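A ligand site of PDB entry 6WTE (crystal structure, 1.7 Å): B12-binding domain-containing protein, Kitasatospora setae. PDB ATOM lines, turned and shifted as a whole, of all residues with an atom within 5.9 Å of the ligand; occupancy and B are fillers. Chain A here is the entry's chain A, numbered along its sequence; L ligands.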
ATOM      1  N   CYS A 227       8.344  -4.084   5.614  1.00  0.00           N
ATOM      2  CA  CYS A 227       8.570  -3.217   6.758  1.00  0.00           C
ATOM      3  C   CYS A 227       7.645  -2.022   6.643  1.00  0.00           C
ATOM      4  O   CYS A 227       7.599  -1.383   5.595  1.00  0.00           O
ATOM      5  CB  CYS A 227      10.018  -2.728   6.859  1.00  0.00           C
ATOM      6  SG  CYS A 227      10.297  -1.734   8.375  1.00  0.00           S
ATOM      7  N   ALA A 228       6.932  -1.716   7.730  1.00  0.00           N
ATOM      8  CA  ALA A 228       5.983  -0.609   7.731  1.00  0.00           C
ATOM      9  C   ALA A 228       6.597   0.717   8.162  1.00  0.00           C
ATOM     10  O   ALA A 228       5.899   1.736   8.109  1.00  0.00           O
ATOM     11  CB  ALA A 228       4.792  -0.945   8.627  1.00  0.00           C
ATOM     12  N   TYR A 229       7.856   0.749   8.573  1.00  0.00           N
ATOM     13  CA  TYR A 229       8.489   2.019   8.924  1.00  0.00           C
ATOM     14  C   TYR A 229       9.030   2.681   7.646  1.00  0.00           C
ATOM     15  O   TYR A 229       8.754   2.237   6.526  1.00  0.00           O
ATOM     16  CB  TYR A 229       9.544   1.807  10.005  1.00  0.00           C
ATOM     17  CG  TYR A 229       8.961   1.529  11.374  1.00  0.00           C
ATOM     18  CD1 TYR A 229       7.589   1.673  11.608  1.00  0.00           C
ATOM     19  CD2 TYR A 229       9.754   1.131  12.429  1.00  0.00           C
ATOM     20  CE1 TYR A 229       7.046   1.425  12.853  1.00  0.00           C
ATOM     21  CE2 TYR A 229       9.225   0.876  13.681  1.00  0.00           C
ATOM     22  CZ  TYR A 229       7.862   1.017  13.883  1.00  0.00           C
ATOM     23  OH  TYR A 229       7.329   0.772  15.127  1.00  0.00           O
ATOM     24  N   ARG A 230       9.782   3.763   7.797  1.00  0.00           N
ATOM     25  CA  ARG A 230      10.223   4.517   6.624  1.00  0.00           C
ATOM     26  C   ARG A 230      11.561   5.197   6.924  1.00  0.00           C
ATOM     27  O   ARG A 230      11.735   6.402   6.711  1.00  0.00           O
ATOM     28  CB  ARG A 230       9.165   5.523   6.191  1.00  0.00           C
ATOM     29  CG  ARG A 230       9.336   6.080   4.778  1.00  0.00           C
ATOM     30  CD  ARG A 230       9.202   5.005   3.721  1.00  0.00           C
ATOM     31  NE  ARG A 230       7.857   4.426   3.646  1.00  0.00           N
ATOM     32  CZ  ARG A 230       6.884   4.888   2.866  1.00  0.00           C
ATOM     33  NH1 ARG A 230       7.110   5.933   2.080  1.00  0.00           N
ATOM     34  NH2 ARG A 230       5.692   4.311   2.862  1.00  0.00           N
ATOM     35  N   CYS A 231      12.514   4.424   7.427  1.00  0.00           N
ATOM     36  CA  CYS A 231      13.809   4.995   7.803  1.00  0.00           C
ATOM     37  C   CYS A 231      14.492   5.584   6.577  1.00  0.00           C
ATOM     38  O   CYS A 231      14.488   5.013   5.488  1.00  0.00           O
ATOM     39  CB  CYS A 231      14.681   3.914   8.455  1.00  0.00           C
ATOM     40  SG  CYS A 231      13.977   3.292  10.004  1.00  0.00           S
ATOM     41  N   HIS A 233      17.377   5.988   5.416  1.00  0.00           N
ATOM     42  CA  HIS A 233      18.518   5.349   4.762  1.00  0.00           C
ATOM     43  C   HIS A 233      18.163   4.025   4.102  1.00  0.00           C
ATOM     44  O   HIS A 233      19.030   3.424   3.449  1.00  0.00           O
ATOM     45  CB  HIS A 233      19.633   5.090   5.779  1.00  0.00           C
ATOM     46  CG  HIS A 233      19.300   4.016   6.769  1.00  0.00           C
ATOM     47  ND1 HIS A 233      18.185   4.062   7.577  1.00  0.00           N
ATOM     48  CD2 HIS A 233      19.919   2.846   7.050  1.00  0.00           C
ATOM     49  CE1 HIS A 233      18.145   2.980   8.333  1.00  0.00           C
ATOM     50  NE2 HIS A 233      19.191   2.218   8.033  1.00  0.00           N
ATOM     51  N   CYS A 234      16.938   3.542   4.245  1.00  0.00           N
ATOM     52  CA  CYS A 234      16.651   2.130   4.085  1.00  0.00           C
ATOM     53  C   CYS A 234      15.861   1.846   2.820  1.00  0.00           C
ATOM     54  O   CYS A 234      14.820   2.472   2.576  1.00  0.00           O
ATOM     55  CB  CYS A 234      15.873   1.602   5.289  1.00  0.00           C
ATOM     56  SG  CYS A 234      15.757  -0.168   5.247  1.00  0.00           S
ATOM     57  N   VAL A 235      16.328   0.857   2.045  1.00  0.00           N
ATOM     58  CA  VAL A 235      15.672   0.449   0.809  1.00  0.00           C
ATOM     59  C   VAL A 235      14.525  -0.525   1.008  1.00  0.00           C
ATOM     60  O   VAL A 235      13.785  -0.799   0.052  1.00  0.00           O
ATOM     61  CB  VAL A 235      16.652  -0.251  -0.156  1.00  0.00           C
ATOM     62  CG1 VAL A 235      17.799   0.697  -0.530  1.00  0.00           C
ATOM     63  CG2 VAL A 235      17.206  -1.536   0.487  1.00  0.00           C
ATOM     64  N   GLU A 236      14.351  -1.071   2.209  1.00  0.00           N
ATOM     65  CA  GLU A 236      13.503  -2.257   2.353  1.00  0.00           C
ATOM     66  C   GLU A 236      12.007  -1.969   2.306  1.00  0.00           C
ATOM     67  O   GLU A 236      11.261  -2.789   1.747  1.00  0.00           O
ATOM     68  CB  GLU A 236      13.862  -3.021   3.630  1.00  0.00           C
ATOM     69  CG  GLU A 236      15.328  -3.436   3.626  1.00  0.00           C
ATOM     70  CD  GLU A 236      15.677  -4.507   4.626  1.00  0.00           C
ATOM     71  OE1 GLU A 236      14.778  -5.294   5.025  1.00  0.00           O
ATOM     72  OE2 GLU A 236      16.871  -4.584   5.002  1.00  0.00           O
ATOM     73  N   PRO A 237      11.496  -0.866   2.876  1.00  0.00           N
ATOM     74  CA  PRO A 237      10.064  -0.600   2.675  1.00  0.00           C
ATOM     75  C   PRO A 237       9.679  -0.591   1.205  1.00  0.00           C
ATOM     76  O   PRO A 237       8.661  -1.178   0.821  1.00  0.00           O
ATOM     77  CB  PRO A 237       9.862   0.764   3.344  1.00  0.00           C
ATOM     78  CG  PRO A 237      10.885   0.771   4.444  1.00  0.00           C
ATOM     79  CD  PRO A 237      12.085   0.064   3.866  1.00  0.00           C
ATOM     80  N   SER A 272      12.799  -8.169   7.621  1.00  0.00           N
ATOM     81  CA  SER A 272      13.413  -6.848   7.738  1.00  0.00           C
ATOM     82  C   SER A 272      13.791  -6.561   9.181  1.00  0.00           C
ATOM     83  O   SER A 272      14.925  -6.149   9.479  1.00  0.00           O
ATOM     84  CB  SER A 272      12.462  -5.783   7.185  1.00  0.00           C
ATOM     85  OG  SER A 272      12.360  -5.892   5.775  1.00  0.00           O
ATOM     86  N   GLU A 273      12.859  -6.775  10.106  1.00  0.00           N
ATOM     87  CA  GLU A 273      13.110  -6.628  11.541  1.00  0.00           C
ATOM     88  C   GLU A 273      12.258  -7.671  12.261  1.00  0.00           C
ATOM     89  O   GLU A 273      11.037  -7.630  12.138  1.00  0.00           O
ATOM     90  CB  GLU A 273      12.752  -5.219  12.044  1.00  0.00           C
ATOM     91  CG  GLU A 273      13.308  -4.065  11.215  1.00  0.00           C
ATOM     92  CD  GLU A 273      14.788  -3.849  11.443  1.00  0.00           C
ATOM     93  OE1 GLU A 273      15.350  -4.470  12.362  1.00  0.00           O
ATOM     94  OE2 GLU A 273      15.379  -3.025  10.714  1.00  0.00           O
ATOM     95  N   LEU A 276       9.566  -6.197  14.836  1.00  0.00           N
ATOM     96  CA  LEU A 276       8.443  -5.404  14.369  1.00  0.00           C
ATOM     97  C   LEU A 276       7.342  -6.363  13.933  1.00  0.00           C
ATOM     98  O   LEU A 276       7.609  -7.517  13.594  1.00  0.00           O
ATOM     99  CB  LEU A 276       8.851  -4.456  13.242  1.00  0.00           C
ATOM    100  CG  LEU A 276       9.920  -3.429  13.659  1.00  0.00           C
ATOM    101  CD1 LEU A 276      10.163  -2.414  12.542  1.00  0.00           C
ATOM    102  CD2 LEU A 276       9.523  -2.708  14.952  1.00  0.00           C
ATOM    103  N   TYR A 308      17.539 -10.410  14.063  1.00  0.00           N
ATOM    104  CA  TYR A 308      17.877  -9.013  13.860  1.00  0.00           C
ATOM    105  C   TYR A 308      16.681  -8.164  14.272  1.00  0.00           C
ATOM    106  O   TYR A 308      15.555  -8.439  13.846  1.00  0.00           O
ATOM    107  CB  TYR A 308      18.246  -8.718  12.391  1.00  0.00           C
ATOM    108  CG  TYR A 308      18.844  -7.336  12.222  1.00  0.00           C
ATOM    109  CD1 TYR A 308      18.031  -6.224  12.032  1.00  0.00           C
ATOM    110  CD2 TYR A 308      20.218  -7.144  12.269  1.00  0.00           C
ATOM    111  CE1 TYR A 308      18.572  -4.958  11.888  1.00  0.00           C
ATOM    112  CE2 TYR A 308      20.762  -5.888  12.133  1.00  0.00           C
ATOM    113  CZ  TYR A 308      19.945  -4.798  11.941  1.00  0.00           C
ATOM    114  OH  TYR A 308      20.491  -3.550  11.794  1.00  0.00           O
ATOM    115  N   GLN A 310      15.064  -4.178  15.928  1.00  0.00           N
ATOM    116  CA  GLN A 310      15.136  -2.777  16.310  1.00  0.00           C
ATOM    117  C   GLN A 310      15.106  -2.679  17.828  1.00  0.00           C
ATOM    118  O   GLN A 310      14.751  -3.641  18.520  1.00  0.00           O
ATOM    119  CB  GLN A 310      13.990  -1.990  15.703  1.00  0.00           C
ATOM    120  CG  GLN A 310      14.130  -1.785  14.193  1.00  0.00           C
ATOM    121  CD  GLN A 310      15.340  -0.930  13.861  1.00  0.00           C
ATOM    122  OE1 GLN A 310      15.371   0.263  14.154  1.00  0.00           O
ATOM    123  NE2 GLN A 310      16.355  -1.551  13.266  1.00  0.00           N
ATOM    124  N   ASP A 335      21.831   2.169  15.710  1.00  0.00           N
ATOM    125  CA  ASP A 335      22.261   3.109  14.671  1.00  0.00           C
ATOM    126  C   ASP A 335      22.851   4.412  15.215  1.00  0.00           C
ATOM    127  O   ASP A 335      23.898   4.845  14.725  1.00  0.00           O
ATOM    128  CB  ASP A 335      21.105   3.381  13.702  1.00  0.00           C
ATOM    129  CG  ASP A 335      20.857   2.203  12.770  1.00  0.00           C
ATOM    130  OD1 ASP A 335      21.821   1.427  12.551  1.00  0.00           O
ATOM    131  OD2 ASP A 335      19.732   2.043  12.276  1.00  0.00           O
ATOM    132  N   LYS A 346      15.546   7.551  11.713  1.00  0.00           N
ATOM    133  CA  LYS A 346      14.949   6.288  12.140  1.00  0.00           C
ATOM    134  C   LYS A 346      13.503   6.597  12.534  1.00  0.00           C
ATOM    135  O   LYS A 346      13.206   6.871  13.703  1.00  0.00           O
ATOM    136  CB  LYS A 346      15.745   5.668  13.281  1.00  0.00           C
ATOM    137  CG  LYS A 346      17.167   5.267  12.899  1.00  0.00           C
ATOM    138  CD  LYS A 346      17.185   4.173  11.839  1.00  0.00           C
ATOM    139  CE  LYS A 346      16.601   2.875  12.381  1.00  0.00           C
ATOM    140  NZ  LYS A 346      17.480   2.212  13.405  1.00  0.00           N
ATOM    141  N   VAL A 347      12.610   6.578  11.547  1.00  0.00           N
ATOM    142  CA  VAL A 347      11.247   7.074  11.759  1.00  0.00           C
ATOM    143  C   VAL A 347      10.224   6.092  11.199  1.00  0.00           C
ATOM    144  O   VAL A 347      10.508   5.289  10.308  1.00  0.00           O
ATOM    145  CB  VAL A 347      11.044   8.440  11.098  1.00  0.00           C
ATOM    146  CG1 VAL A 347      12.036   9.448  11.635  1.00  0.00           C
ATOM    147  CG2 VAL A 347      11.206   8.261   9.604  1.00  0.00           C
ATOM    148  N   TYR A 354      10.749   6.123  17.102  1.00  0.00           N
ATOM    149  CA  TYR A 354      10.027   5.042  17.759  1.00  0.00           C
ATOM    150  C   TYR A 354      10.871   4.334  18.813  1.00  0.00           C
ATOM    151  O   TYR A 354      10.462   3.273  19.298  1.00  0.00           O
ATOM    152  CB  TYR A 354       9.508   4.034  16.721  1.00  0.00           C
ATOM    153  CG  TYR A 354      10.580   3.467  15.810  1.00  0.00           C
ATOM    154  CD1 TYR A 354      10.934   4.123  14.637  1.00  0.00           C
ATOM    155  CD2 TYR A 354      11.218   2.278  16.117  1.00  0.00           C
ATOM    156  CE1 TYR A 354      11.912   3.614  13.796  1.00  0.00           C
ATOM    157  CE2 TYR A 354      12.202   1.748  15.282  1.00  0.00           C
ATOM    158  CZ  TYR A 354      12.540   2.429  14.125  1.00  0.00           C
ATOM    159  OH  TYR A 354      13.518   1.926  13.305  1.00  0.00           O
HETATM  160 FE1  LIG L   1      13.912   1.093   9.420  1.00  0.00          FE
HETATM  161 FE2  LIG L   1      12.343  -0.945   8.439  1.00  0.00          FE
HETATM  162 FE3  LIG L   1      14.667  -1.550   9.698  1.00  0.00          FE
HETATM  163 FE4  LIG L   1      14.740  -0.384   7.271  1.00  0.00          FE
HETATM  164  S1  LIG L   1      13.926  -2.450   7.738  1.00  0.00           S
HETATM  165  S2  LIG L   1      15.984   0.186   9.085  1.00  0.00           S
HETATM  166  S3  LIG L   1      12.905   0.984   7.361  1.00  0.00           S
HETATM  167  S4  LIG L   1      12.849  -0.515  10.632  1.00  0.00           S
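FE3 of the ligand is bound by OE2 of Glu 273, at 1.9 Å. FE2 of the ligand is bound by SG of Cys 227 (2.2 Å). SG of Cys 234 is bound to FE4 of the ligand. N of Cys 231 sits close to S3 of the ligand (3.5 Å). The side-chain sulfur of Cys 231 binds an iron atom (FE1) of the ligand (2.3 Å). The side-chain hydroxyl (OH) of Tyr 354 lies close to a sulfur (S4) of the ligand, at 3.7 Å.
The side-chain carboxylate of Glu 273 is in hydrogen-bond range of the side-chain amide nitrogen of Gln 310, 3.2 Å away. N of Tyr 229 lies close to SG of Cys 227, 3.5 Å away. The side-chain sulfur (SG) of Cys 234 sits close to the backbone NH (N) of Glu 236, at 3.5 Å. The side-chain sulfur of Cys 231 lies close to the side-chain hydroxyl of Tyr 354, at 3.6 Å. OE1 of Gln 310 lies within hydrogen-bond range of OH of Tyr 354, at 2.6 Å. OG of Ser 272 is in hydrogen-bond range of OE1 of Glu 236 (2.6 Å). NZ of Lys 346 sits at hydrogen-bond distance from OE1 of Gln 310 (3.0 Å).
Residues that only touch the ligand: Tyr 229, His 233, Pro 237, Ser 272, Leu 276 and Gln 310. Hydrophobic or aromatic side chains within 4 Å of the ligand: Tyr 229, His 233, Pro 237 and Leu 276. Within 4 Å of the ligand: Cys 227, Tyr 229, Cys 231, His 233, Cys 234, Pro 237, Ser 272, Glu 273, Leu 276, Gln 310 and Tyr 354. The nearest printed residue that does not touch the ligand is Glu 236 (4.02 Å).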
